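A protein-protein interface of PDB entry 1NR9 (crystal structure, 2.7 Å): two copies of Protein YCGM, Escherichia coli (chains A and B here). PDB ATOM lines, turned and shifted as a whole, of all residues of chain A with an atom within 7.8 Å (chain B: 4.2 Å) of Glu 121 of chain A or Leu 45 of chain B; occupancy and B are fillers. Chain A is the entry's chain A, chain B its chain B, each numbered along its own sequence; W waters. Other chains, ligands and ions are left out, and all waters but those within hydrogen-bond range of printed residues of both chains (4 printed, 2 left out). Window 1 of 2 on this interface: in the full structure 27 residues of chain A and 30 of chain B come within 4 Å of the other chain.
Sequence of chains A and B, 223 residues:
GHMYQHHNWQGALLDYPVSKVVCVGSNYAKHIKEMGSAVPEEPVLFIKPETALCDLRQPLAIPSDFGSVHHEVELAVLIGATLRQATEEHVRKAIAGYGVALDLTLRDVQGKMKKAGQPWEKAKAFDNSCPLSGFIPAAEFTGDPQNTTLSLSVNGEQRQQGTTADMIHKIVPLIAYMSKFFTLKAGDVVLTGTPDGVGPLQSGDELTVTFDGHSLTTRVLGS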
ATOM      1  N   PHE A  46      16.539 -14.910 -13.877  1.00  0.00           N
ATOM      2  CA  PHE A  46      16.874 -13.512 -14.151  1.00  0.00           C
ATOM      3  C   PHE A  46      15.554 -12.749 -14.308  1.00  0.00           C
ATOM      4  O   PHE A  46      14.504 -13.367 -14.536  1.00  0.00           O
ATOM      5  CB  PHE A  46      17.756 -13.388 -15.402  1.00  0.00           C
ATOM      6  CG  PHE A  46      17.064 -13.746 -16.681  1.00  0.00           C
ATOM      7  CD1 PHE A  46      16.366 -12.787 -17.400  1.00  0.00           C
ATOM      8  CD2 PHE A  46      17.127 -15.042 -17.178  1.00  0.00           C
ATOM      9  CE1 PHE A  46      15.734 -13.114 -18.598  1.00  0.00           C
ATOM     10  CE2 PHE A  46      16.500 -15.378 -18.368  1.00  0.00           C
ATOM     11  CZ  PHE A  46      15.803 -14.409 -19.083  1.00  0.00           C
ATOM     12  N   ILE A  47      15.591 -11.422 -14.181  1.00  0.00           N
ATOM     13  CA  ILE A  47      14.359 -10.635 -14.272  1.00  0.00           C
ATOM     14  C   ILE A  47      14.328  -9.452 -15.246  1.00  0.00           C
ATOM     15  O   ILE A  47      15.248  -8.632 -15.289  1.00  0.00           O
ATOM     16  CB  ILE A  47      13.972 -10.076 -12.893  1.00  0.00           C
ATOM     17  CG1 ILE A  47      14.045 -11.179 -11.837  1.00  0.00           C
ATOM     18  CG2 ILE A  47      12.573  -9.485 -12.959  1.00  0.00           C
ATOM     19  CD1 ILE A  47      13.837 -10.674 -10.403  1.00  0.00           C
ATOM     20  N   LYS A  48      13.248  -9.358 -16.013  1.00  0.00           N
ATOM     21  CA  LYS A  48      13.076  -8.248 -16.943  1.00  0.00           C
ATOM     22  C   LYS A  48      12.213  -7.193 -16.223  1.00  0.00           C
ATOM     23  O   LYS A  48      11.192  -7.516 -15.611  1.00  0.00           O
ATOM     24  CB  LYS A  48      12.385  -8.724 -18.223  1.00  0.00           C
ATOM     25  CG  LYS A  48      13.244  -9.574 -19.128  1.00  0.00           C
ATOM     26  CD  LYS A  48      12.456  -9.983 -20.350  1.00  0.00           C
ATOM     27  CE  LYS A  48      13.261 -10.903 -21.270  1.00  0.00           C
ATOM     28  NZ  LYS A  48      14.343 -10.198 -22.037  1.00  0.00           N
ATOM     29  N   PRO A  49      12.614  -5.915 -16.281  1.00  0.00           N
ATOM     30  CA  PRO A  49      11.848  -4.854 -15.613  1.00  0.00           C
ATOM     31  C   PRO A  49      10.621  -4.388 -16.391  1.00  0.00           C
ATOM     32  O   PRO A  49      10.432  -4.774 -17.534  1.00  0.00           O
ATOM     33  CB  PRO A  49      12.887  -3.762 -15.442  1.00  0.00           C
ATOM     34  CG  PRO A  49      13.646  -3.866 -16.764  1.00  0.00           C
ATOM     35  CD  PRO A  49      13.838  -5.374 -16.901  1.00  0.00           C
ATOM     36  N   LEU A 106      20.185  -9.846 -26.101  1.00  0.00           N
ATOM     37  CA  LEU A 106      21.369  -9.374 -26.818  1.00  0.00           C
ATOM     38  C   LEU A 106      22.502 -10.404 -26.625  1.00  0.00           C
ATOM     39  O   LEU A 106      23.336 -10.251 -25.719  1.00  0.00           O
ATOM     40  CB  LEU A 106      21.807  -8.013 -26.261  1.00  0.00           C
ATOM     41  CG  LEU A 106      20.893  -6.814 -26.553  1.00  0.00           C
ATOM     42  CD1 LEU A 106      21.433  -5.569 -25.863  1.00  0.00           C
ATOM     43  CD2 LEU A 106      20.819  -6.581 -28.065  1.00  0.00           C
ATOM     44  N   VAL A 109      26.318  -9.339 -26.267  1.00  0.00           N
ATOM     45  CA  VAL A 109      26.496  -8.751 -24.947  1.00  0.00           C
ATOM     46  C   VAL A 109      26.465  -9.779 -23.826  1.00  0.00           C
ATOM     47  O   VAL A 109      27.236  -9.684 -22.865  1.00  0.00           O
ATOM     48  CB  VAL A 109      25.399  -7.732 -24.653  1.00  0.00           C
ATOM     49  CG1 VAL A 109      25.545  -7.227 -23.225  1.00  0.00           C
ATOM     50  CG2 VAL A 109      25.457  -6.591 -25.667  1.00  0.00           C
ATOM     51  N   GLN A 110      25.562 -10.747 -23.943  1.00  0.00           N
ATOM     52  CA  GLN A 110      25.432 -11.787 -22.933  1.00  0.00           C
ATOM     53  C   GLN A 110      26.706 -12.611 -22.841  1.00  0.00           C
ATOM     54  O   GLN A 110      27.176 -12.923 -21.744  1.00  0.00           O
ATOM     55  CB  GLN A 110      24.273 -12.712 -23.265  1.00  0.00           C
ATOM     56  CG  GLN A 110      23.580 -13.248 -22.037  1.00  0.00           C
ATOM     57  CD  GLN A 110      22.909 -14.567 -22.288  1.00  0.00           C
ATOM     58  OE1 GLN A 110      22.304 -14.776 -23.336  1.00  0.00           O
ATOM     59  NE2 GLN A 110      23.000 -15.472 -21.317  1.00  0.00           N
ATOM     60  N   MET A 113      29.091 -10.966 -20.898  1.00  0.00           N
ATOM     61  CA  MET A 113      28.662 -11.048 -19.501  1.00  0.00           C
ATOM     62  C   MET A 113      29.003 -12.408 -18.877  1.00  0.00           C
ATOM     63  O   MET A 113      29.643 -12.462 -17.827  1.00  0.00           O
ATOM     64  CB  MET A 113      27.152 -10.783 -19.385  1.00  0.00           C
ATOM     65  CG  MET A 113      26.682  -9.422 -19.931  1.00  0.00           C
ATOM     66  SD  MET A 113      27.334  -7.791 -19.029  1.00  0.00           S
ATOM     67  CE  MET A 113      28.857  -7.388 -20.170  1.00  0.00           C
ATOM     68  N   GLN A 118      29.173 -11.530 -15.059  1.00  0.00           N
ATOM     69  CA  GLN A 118      28.560 -10.245 -14.767  1.00  0.00           C
ATOM     70  C   GLN A 118      27.043 -10.264 -14.900  1.00  0.00           C
ATOM     71  O   GLN A 118      26.475 -11.157 -15.539  1.00  0.00           O
ATOM     72  CB  GLN A 118      29.134  -9.180 -15.691  1.00  0.00           C
ATOM     73  CG  GLN A 118      30.616  -9.028 -15.592  1.00  0.00           C
ATOM     74  CD  GLN A 118      31.087  -7.700 -16.142  1.00  0.00           C
ATOM     75  OE1 GLN A 118      30.625  -7.252 -17.195  1.00  0.00           O
ATOM     76  NE2 GLN A 118      32.016  -7.059 -15.434  1.00  0.00           N
ATOM     77  N   PRO A 119      26.367  -9.257 -14.309  1.00  0.00           N
ATOM     78  CA  PRO A 119      24.911  -9.187 -14.376  1.00  0.00           C
ATOM     79  C   PRO A 119      24.467  -9.373 -15.823  1.00  0.00           C
ATOM     80  O   PRO A 119      25.226  -9.124 -16.751  1.00  0.00           O
ATOM     81  CB  PRO A 119      24.611  -7.786 -13.843  1.00  0.00           C
ATOM     82  CG  PRO A 119      25.773  -7.476 -12.964  1.00  0.00           C
ATOM     83  CD  PRO A 119      26.914  -7.999 -13.765  1.00  0.00           C
ATOM     84  N   TRP A 120      23.231  -9.800 -16.007  1.00  0.00           N
ATOM     85  CA  TRP A 120      22.704 -10.043 -17.334  1.00  0.00           C
ATOM     86  C   TRP A 120      21.791  -8.938 -17.840  1.00  0.00           C
ATOM     87  O   TRP A 120      21.447  -8.904 -19.025  1.00  0.00           O
ATOM     88  CB  TRP A 120      21.920 -11.338 -17.310  1.00  0.00           C
ATOM     89  CG  TRP A 120      22.754 -12.556 -17.376  1.00  0.00           C
ATOM     90  CD1 TRP A 120      24.084 -12.678 -17.069  1.00  0.00           C
ATOM     91  CD2 TRP A 120      22.304 -13.852 -17.752  1.00  0.00           C
ATOM     92  NE1 TRP A 120      24.482 -13.982 -17.230  1.00  0.00           N
ATOM     93  CE2 TRP A 120      23.407 -14.721 -17.646  1.00  0.00           C
ATOM     94  CE3 TRP A 120      21.071 -14.363 -18.166  1.00  0.00           C
ATOM     95  CZ2 TRP A 120      23.315 -16.076 -17.946  1.00  0.00           C
ATOM     96  CZ3 TRP A 120      20.979 -15.711 -18.465  1.00  0.00           C
ATOM     97  CH2 TRP A 120      22.097 -16.554 -18.349  1.00  0.00           C
ATOM     98  N   GLU A 121      21.401  -8.040 -16.943  1.00  0.00           N
ATOM     99  CA  GLU A 121      20.482  -6.970 -17.304  1.00  0.00           C
ATOM    100  C   GLU A 121      20.744  -6.292 -18.655  1.00  0.00           C
ATOM    101  O   GLU A 121      19.794  -5.963 -19.379  1.00  0.00           O
ATOM    102  CB  GLU A 121      20.407  -5.928 -16.173  1.00  0.00           C
ATOM    103  CG  GLU A 121      19.563  -6.385 -14.957  1.00  0.00           C
ATOM    104  CD  GLU A 121      20.274  -7.408 -14.059  1.00  0.00           C
ATOM    105  OE1 GLU A 121      21.052  -8.236 -14.587  1.00  0.00           O
ATOM    106  OE2 GLU A 121      20.050  -7.391 -12.828  1.00  0.00           O
ATOM    107  N   LYS A 122      22.010  -6.102 -19.016  1.00  0.00           N
ATOM    108  CA  LYS A 122      22.306  -5.450 -20.283  1.00  0.00           C
ATOM    109  C   LYS A 122      21.838  -6.278 -21.465  1.00  0.00           C
ATOM    110  O   LYS A 122      21.325  -5.743 -22.443  1.00  0.00           O
ATOM    111  CB  LYS A 122      23.801  -5.182 -20.421  1.00  0.00           C
ATOM    112  CG  LYS A 122      24.308  -4.049 -19.564  1.00  0.00           C
ATOM    113  CD  LYS A 122      25.798  -3.871 -19.768  1.00  0.00           C
ATOM    114  CE  LYS A 122      26.372  -2.790 -18.865  1.00  0.00           C
ATOM    115  NZ  LYS A 122      27.849  -2.667 -19.067  1.00  0.00           N
ATOM    116  N   ALA A 123      22.000  -7.589 -21.366  1.00  0.00           N
ATOM    117  CA  ALA A 123      21.628  -8.484 -22.448  1.00  0.00           C
ATOM    118  C   ALA A 123      20.187  -8.958 -22.407  1.00  0.00           C
ATOM    119  O   ALA A 123      19.604  -9.248 -23.452  1.00  0.00           O
ATOM    120  CB  ALA A 123      22.559  -9.696 -22.447  1.00  0.00           C
ATOM    121  N   LYS A 124      19.612  -9.044 -21.211  1.00  0.00           N
ATOM    122  CA  LYS A 124      18.247  -9.543 -21.053  1.00  0.00           C
ATOM    123  C   LYS A 124      17.201  -8.546 -20.564  1.00  0.00           C
ATOM    124  O   LYS A 124      16.004  -8.863 -20.555  1.00  0.00           O
ATOM    125  CB  LYS A 124      18.249 -10.737 -20.091  1.00  0.00           C
ATOM    126  CG  LYS A 124      18.806 -12.035 -20.659  1.00  0.00           C
ATOM    127  CD  LYS A 124      17.795 -12.740 -21.544  1.00  0.00           C
ATOM    128  CE  LYS A 124      18.302 -14.108 -21.946  1.00  0.00           C
ATOM    129  NZ  LYS A 124      17.291 -14.894 -22.720  1.00  0.00           N
ATOM    130  N   ALA A 125      17.614  -7.351 -20.160  1.00  0.00           N
ATOM    131  CA  ALA A 125      16.615  -6.429 -19.637  1.00  0.00           C
ATOM    132  C   ALA A 125      16.458  -5.091 -20.327  1.00  0.00           C
ATOM    133  O   ALA A 125      15.738  -4.232 -19.821  1.00  0.00           O
ATOM    134  CB  ALA A 125      16.856  -6.212 -18.140  1.00  0.00           C
ATOM    135  N   PHE A 126      17.114  -4.902 -21.471  1.00  0.00           N
ATOM    136  CA  PHE A 126      17.017  -3.624 -22.189  1.00  0.00           C
ATOM    137  C   PHE A 126      15.562  -3.270 -22.507  1.00  0.00           C
ATOM    138  O   PHE A 126      14.666  -4.099 -22.340  1.00  0.00           O
ATOM    139  CB  PHE A 126      17.860  -3.648 -23.480  1.00  0.00           C
ATOM    140  CG  PHE A 126      17.508  -4.762 -24.423  1.00  0.00           C
ATOM    141  CD1 PHE A 126      18.127  -6.005 -24.316  1.00  0.00           C
ATOM    142  CD2 PHE A 126      16.533  -4.578 -25.400  1.00  0.00           C
ATOM    143  CE1 PHE A 126      17.776  -7.058 -25.174  1.00  0.00           C
ATOM    144  CE2 PHE A 126      16.177  -5.616 -26.255  1.00  0.00           C
ATOM    145  CZ  PHE A 126      16.799  -6.863 -26.143  1.00  0.00           C
ATOM    146  N   ASP A 127      15.329  -2.040 -22.952  1.00  0.00           N
ATOM    147  CA  ASP A 127      13.972  -1.588 -23.252  1.00  0.00           C
ATOM    148  C   ASP A 127      13.253  -2.472 -24.250  1.00  0.00           C
ATOM    149  O   ASP A 127      13.821  -2.878 -25.262  1.00  0.00           O
ATOM    150  CB  ASP A 127      13.977  -0.153 -23.790  1.00  0.00           C
ATOM    151  CG  ASP A 127      14.478   0.856 -22.777  1.00  0.00           C
ATOM    152  OD1 ASP A 127      14.425   0.564 -21.566  1.00  0.00           O
ATOM    153  OD2 ASP A 127      14.910   1.955 -23.198  1.00  0.00           O
ATOM    154  N   SER A 129      12.393  -5.575 -24.239  1.00  0.00           N
ATOM    155  CA  SER A 129      13.113  -6.820 -24.480  1.00  0.00           C
ATOM    156  C   SER A 129      12.167  -7.961 -24.162  1.00  0.00           C
ATOM    157  O   SER A 129      12.598  -9.106 -23.994  1.00  0.00           O
ATOM    158  CB  SER A 129      14.326  -6.917 -23.568  1.00  0.00           C
ATOM    159  OG  SER A 129      13.905  -7.022 -22.219  1.00  0.00           O
ATOM    160  N   CYS B  23      21.498  -0.436 -10.445  1.00  0.00           N
ATOM    161  CA  CYS B  23      22.666  -0.231  -9.583  1.00  0.00           C
ATOM    162  C   CYS B  23      23.998  -0.543 -10.245  1.00  0.00           C
ATOM    163  O   CYS B  23      24.059  -1.263 -11.242  1.00  0.00           O
ATOM    164  CB  CYS B  23      22.550  -1.104  -8.327  1.00  0.00           C
ATOM    165  SG  CYS B  23      20.871  -1.402  -7.714  1.00  0.00           S
ATOM    166  N   PRO B  43      30.544   0.872 -16.445  1.00  0.00           N
ATOM    167  CA  PRO B  43      29.781   0.406 -15.286  1.00  0.00           C
ATOM    168  C   PRO B  43      29.143  -0.962 -15.476  1.00  0.00           C
ATOM    169  O   PRO B  43      28.637  -1.281 -16.561  1.00  0.00           O
ATOM    170  CB  PRO B  43      28.710   1.485 -15.113  1.00  0.00           C
ATOM    171  CG  PRO B  43      29.373   2.704 -15.630  1.00  0.00           C
ATOM    172  CD  PRO B  43      30.085   2.209 -16.858  1.00  0.00           C
ATOM    173  N   VAL B  44      29.190  -1.762 -14.409  1.00  0.00           N
ATOM    174  CA  VAL B  44      28.577  -3.086 -14.366  1.00  0.00           C
ATOM    175  C   VAL B  44      27.140  -2.777 -13.942  1.00  0.00           C
ATOM    176  O   VAL B  44      26.941  -2.066 -12.958  1.00  0.00           O
ATOM    177  CB  VAL B  44      29.238  -3.957 -13.284  1.00  0.00           C
ATOM    178  CG1 VAL B  44      28.505  -5.272 -13.156  1.00  0.00           C
ATOM    179  CG2 VAL B  44      30.706  -4.187 -13.619  1.00  0.00           C
ATOM    180  N   LEU B  45      26.136  -3.274 -14.659  1.00  0.00           N
ATOM    181  CA  LEU B  45      24.760  -2.951 -14.274  1.00  0.00           C
ATOM    182  C   LEU B  45      23.805  -4.118 -14.028  1.00  0.00           C
ATOM    183  O   LEU B  45      23.703  -5.044 -14.836  1.00  0.00           O
ATOM    184  CB  LEU B  45      24.121  -2.030 -15.323  1.00  0.00           C
ATOM    185  CG  LEU B  45      24.865  -0.762 -15.757  1.00  0.00           C
ATOM    186  CD1 LEU B  45      24.012  -0.033 -16.793  1.00  0.00           C
ATOM    187  CD2 LEU B  45      25.166   0.131 -14.555  1.00  0.00           C
ATOM    188  N   PHE B  46      23.102  -4.050 -12.898  1.00  0.00           N
ATOM    189  CA  PHE B  46      22.096  -5.038 -12.527  1.00  0.00           C
ATOM    190  C   PHE B  46      20.910  -4.243 -11.986  1.00  0.00           C
ATOM    191  O   PHE B  46      21.025  -3.029 -11.767  1.00  0.00           O
ATOM    192  CB  PHE B  46      22.634  -6.027 -11.488  1.00  0.00           C
ATOM    193  CG  PHE B  46      23.088  -5.392 -10.213  1.00  0.00           C
ATOM    194  CD1 PHE B  46      22.182  -5.121  -9.190  1.00  0.00           C
ATOM    195  CD2 PHE B  46      24.429  -5.062 -10.027  1.00  0.00           C
ATOM    196  CE1 PHE B  46      22.615  -4.531  -7.994  1.00  0.00           C
ATOM    197  CE2 PHE B  46      24.869  -4.472  -8.840  1.00  0.00           C
ATOM    198  CZ  PHE B  46      23.963  -4.207  -7.822  1.00  0.00           C
ATOM    199  N   ILE B  47      19.773  -4.908 -11.784  1.00  0.00           N
ATOM    200  CA  ILE B  47      18.570  -4.237 -11.314  1.00  0.00           C
ATOM    201  C   ILE B  47      17.817  -5.013 -10.237  1.00  0.00           C
ATOM    202  O   ILE B  47      17.718  -6.244 -10.289  1.00  0.00           O
ATOM    203  CB  ILE B  47      17.605  -4.012 -12.481  1.00  0.00           C
ATOM    204  CG1 ILE B  47      18.295  -3.189 -13.568  1.00  0.00           C
ATOM    205  CG2 ILE B  47      16.345  -3.300 -11.996  1.00  0.00           C
ATOM    206  CD1 ILE B  47      17.524  -3.160 -14.928  1.00  0.00           C
ATOM    207  N   GLU B 121      20.405 -12.004 -10.216  1.00  0.00           N
ATOM    208  CA  GLU B 121      19.131 -11.799  -9.534  1.00  0.00           C
ATOM    209  C   GLU B 121      19.025 -12.495  -8.170  1.00  0.00           C
ATOM    210  O   GLU B 121      18.650 -11.863  -7.172  1.00  0.00           O
ATOM    211  CB  GLU B 121      17.959 -12.239 -10.423  1.00  0.00           C
ATOM    212  CG  GLU B 121      17.488 -11.198 -11.434  1.00  0.00           C
ATOM    213  CD  GLU B 121      18.409 -11.045 -12.646  1.00  0.00           C
ATOM    214  OE1 GLU B 121      19.401 -11.812 -12.765  1.00  0.00           O
ATOM    215  OE2 GLU B 121      18.124 -10.158 -13.488  1.00  0.00           O
ATOM    216  N   TYR B 177      24.751   6.912 -18.657  1.00  0.00           N
ATOM    217  CA  TYR B 177      25.106   5.603 -19.176  1.00  0.00           C
ATOM    218  C   TYR B 177      23.933   4.625 -18.978  1.00  0.00           C
ATOM    219  O   TYR B 177      23.442   4.005 -19.934  1.00  0.00           O
ATOM    220  CB  TYR B 177      26.361   5.102 -18.453  1.00  0.00           C
ATOM    221  CG  TYR B 177      26.797   3.718 -18.859  1.00  0.00           C
ATOM    222  CD1 TYR B 177      27.640   3.524 -19.949  1.00  0.00           C
ATOM    223  CD2 TYR B 177      26.309   2.597 -18.189  1.00  0.00           C
ATOM    224  CE1 TYR B 177      27.982   2.252 -20.364  1.00  0.00           C
ATOM    225  CE2 TYR B 177      26.637   1.324 -18.596  1.00  0.00           C
ATOM    226  CZ  TYR B 177      27.474   1.153 -19.688  1.00  0.00           C
ATOM    227  OH  TYR B 177      27.776  -0.124 -20.109  1.00  0.00           O
ATOM    228  N   MET B 178      23.466   4.497 -17.742  1.00  0.00           N
ATOM    229  CA  MET B 178      22.364   3.596 -17.471  1.00  0.00           C
ATOM    230  C   MET B 178      21.209   3.785 -18.431  1.00  0.00           C
ATOM    231  O   MET B 178      20.677   2.799 -18.945  1.00  0.00           O
ATOM    232  CB  MET B 178      21.856   3.764 -16.038  1.00  0.00           C
ATOM    233  CG  MET B 178      22.841   3.298 -14.987  1.00  0.00           C
ATOM    234  SD  MET B 178      22.334   3.812 -13.199  1.00  0.00           S
ATOM    235  CE  MET B 178      23.795   2.965 -12.231  1.00  0.00           C
ATOM    236  N   PHE B 182      18.368   0.849 -20.268  1.00  0.00           N
ATOM    237  CA  PHE B 182      17.000   0.850 -19.783  1.00  0.00           C
ATOM    238  C   PHE B 182      16.626   2.273 -19.469  1.00  0.00           C
ATOM    239  O   PHE B 182      17.374   2.980 -18.781  1.00  0.00           O
ATOM    240  CB  PHE B 182      16.846   0.006 -18.515  1.00  0.00           C
ATOM    241  CG  PHE B 182      18.045  -0.827 -18.187  1.00  0.00           C
ATOM    242  CD1 PHE B 182      19.114  -0.281 -17.494  1.00  0.00           C
ATOM    243  CD2 PHE B 182      18.109  -2.158 -18.584  1.00  0.00           C
ATOM    244  CE1 PHE B 182      20.230  -1.043 -17.205  1.00  0.00           C
ATOM    245  CE2 PHE B 182      19.230  -2.932 -18.298  1.00  0.00           C
ATOM    246  CZ  PHE B 182      20.291  -2.373 -17.606  1.00  0.00           C
HETATM  247  O   HOH W   1      27.140  -5.079 -16.595  1.00  0.00           O
HETATM  248  O   HOH W   2      20.044  -8.325 -10.358  1.00  0.00           O
HETATM  249  O   HOH W   3      21.535 -10.803 -13.933  1.00  0.00           O
HETATM  250  O   HOH W   4      18.155  -9.503 -16.597  1.00  0.00           O
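Printed residues of chain B within 4 Å of Phe 46 of chain A: Glu 121 (3.3 Å). Printed residues of chain B within 4 Å of Ile 47 of chain A: Glu 121. Of chain B, only Leu 45 (3.7 Å), Phe 46 (3.1 Å), Ile 47 (2.7 Å), Glu 121 (3.4 Å) and Phe 182 (3.3 Å) come within 4 Å of Glu 121 of chain A. Of the printed residues of chain A, Pro 43 of chain B touches Lys 122 (3.0 Å). Of the printed residues of chain A, Leu 45 of chain B touches Pro 119 and Glu 121. The nearest printed residue of chain B that does not touch Glu 121 of chain A is Cys 23 of chain B (7.5 Å). The nearest printed residue of chain B that does not touch Phe 46 of chain A is Ile 47 of chain B (7.9 Å).
Water W3 lies within hydrogen-bond range of the side-chain carboxylate (OE1) of Glu 121 of chain B (2.6 Å), the side-chain carboxylate (OE1) of Glu 121 of chain A (2.7 Å) and the backbone NH (N) of Trp 120 of chain A (2.9 Å). Water W2 bridges OE2 of Glu 121 of chain A and O of Ile 47 of chain B. Water W1 lies within hydrogen-bond range of the backbone NH (N) of Leu 45 of chain B and the side-chain sulfur (SD) of Met 113 of chain A. Water W4 bridges the side-chain carboxylate of Glu 121 of chain B (3.2 Å) and the backbone carbonyl oxygen of Ile 47 of chain A (3.3 Å).
Of the 10 printed residues of chain B, 8 touch a printed residue of chain A. Of the 19 printed residues of chain A, 8 touch a printed residue of chain B. Printed residues of chain A that touch a printed residue of chain B: Phe 46, Ile 47, Gln 118, Pro 119, Glu 121, Lys 122, Ala 125 and Asp 127. Hydrophobic or aromatic side chains of chain A within 4 Å of the printed part of chain B: Phe 46, Ile 47 and Pro 119. Among the printed residues, no Asp or Glu carboxylate lies within 4 Å of a Lys or Arg side-chain nitrogen of the other chain.
N of Gln 118 of chain A is in hydrogen-bond range of O of Met 113 of chain A (3.0 Å). N of Cys 23 of chain B sits at hydrogen-bond distance from O of Phe 46 of chain B (2.9 Å).
Phe 46 of chain A touches Glu 121 of chain B. Val 44 of chain B touches Gln 118 of chain A (CG2 to NE2, 3.6 Å). CD of Pro 119 of chain A touches CG1 of Val 44 of chain B (3.2 Å). O of Leu 45 of chain B touches CB of Pro 119 of chain A (3.1 Å). CB of Phe 46 of chain B touches CB of Pro 119 of chain A, 3.5 Å away. Glu 121 of chain A touches Leu 45 of chain B. OE2 of Glu 121 of chain A touches CA of Phe 46 of chain B, 3.1 Å away. Glu 121 of chain A touches Phe 182 of chain B (O to CE2, 3.3 Å). Phe 182 of chain B touches Ala 125 of chain A. Phe 182 of chain B touches Asp 127 of chain A (CA to OD1, 3.1 Å).
N of Ile 47 of chain A sits at hydrogen-bond distance from OE2 of Glu 121 of chain B (2.9 Å). The backbone NH (N) of Ile 47 of chain B lies within hydrogen-bond range of the side-chain carboxylate (OE2) of Glu 121 of chain A, 2.7 Å away. NZ of Lys 122 of chain A lies within hydrogen-bond range of O of Pro 43 of chain B. The side-chain amino group (NZ) of Lys 122 of chain A lies within hydrogen-bond range of the side-chain hydroxyl (OH) of Tyr 177 of chain B (2.7 Å). The side-chain carboxylate (OE2) of Glu 121 of chain B sits close to the side-chain carboxylate (OE2) of Glu 121 of chain A (3.4 Å).
Phe 46 of chain A touches Glu 121 of chain B, and with the chains exchanged Glu 121 of chain A touches Phe 46 of chain B. Ile 47 of chain A touches Glu 121 of chain B, and with the chains exchanged Glu 121 of chain A touches Ile 47 of chain B. Glu 121 of chain A touches its own counterpart, Glu 121 of chain B. Of the 15 pairs that touch across the chains among the printed residues, 5 have their exchanged pair printed and touching as well.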
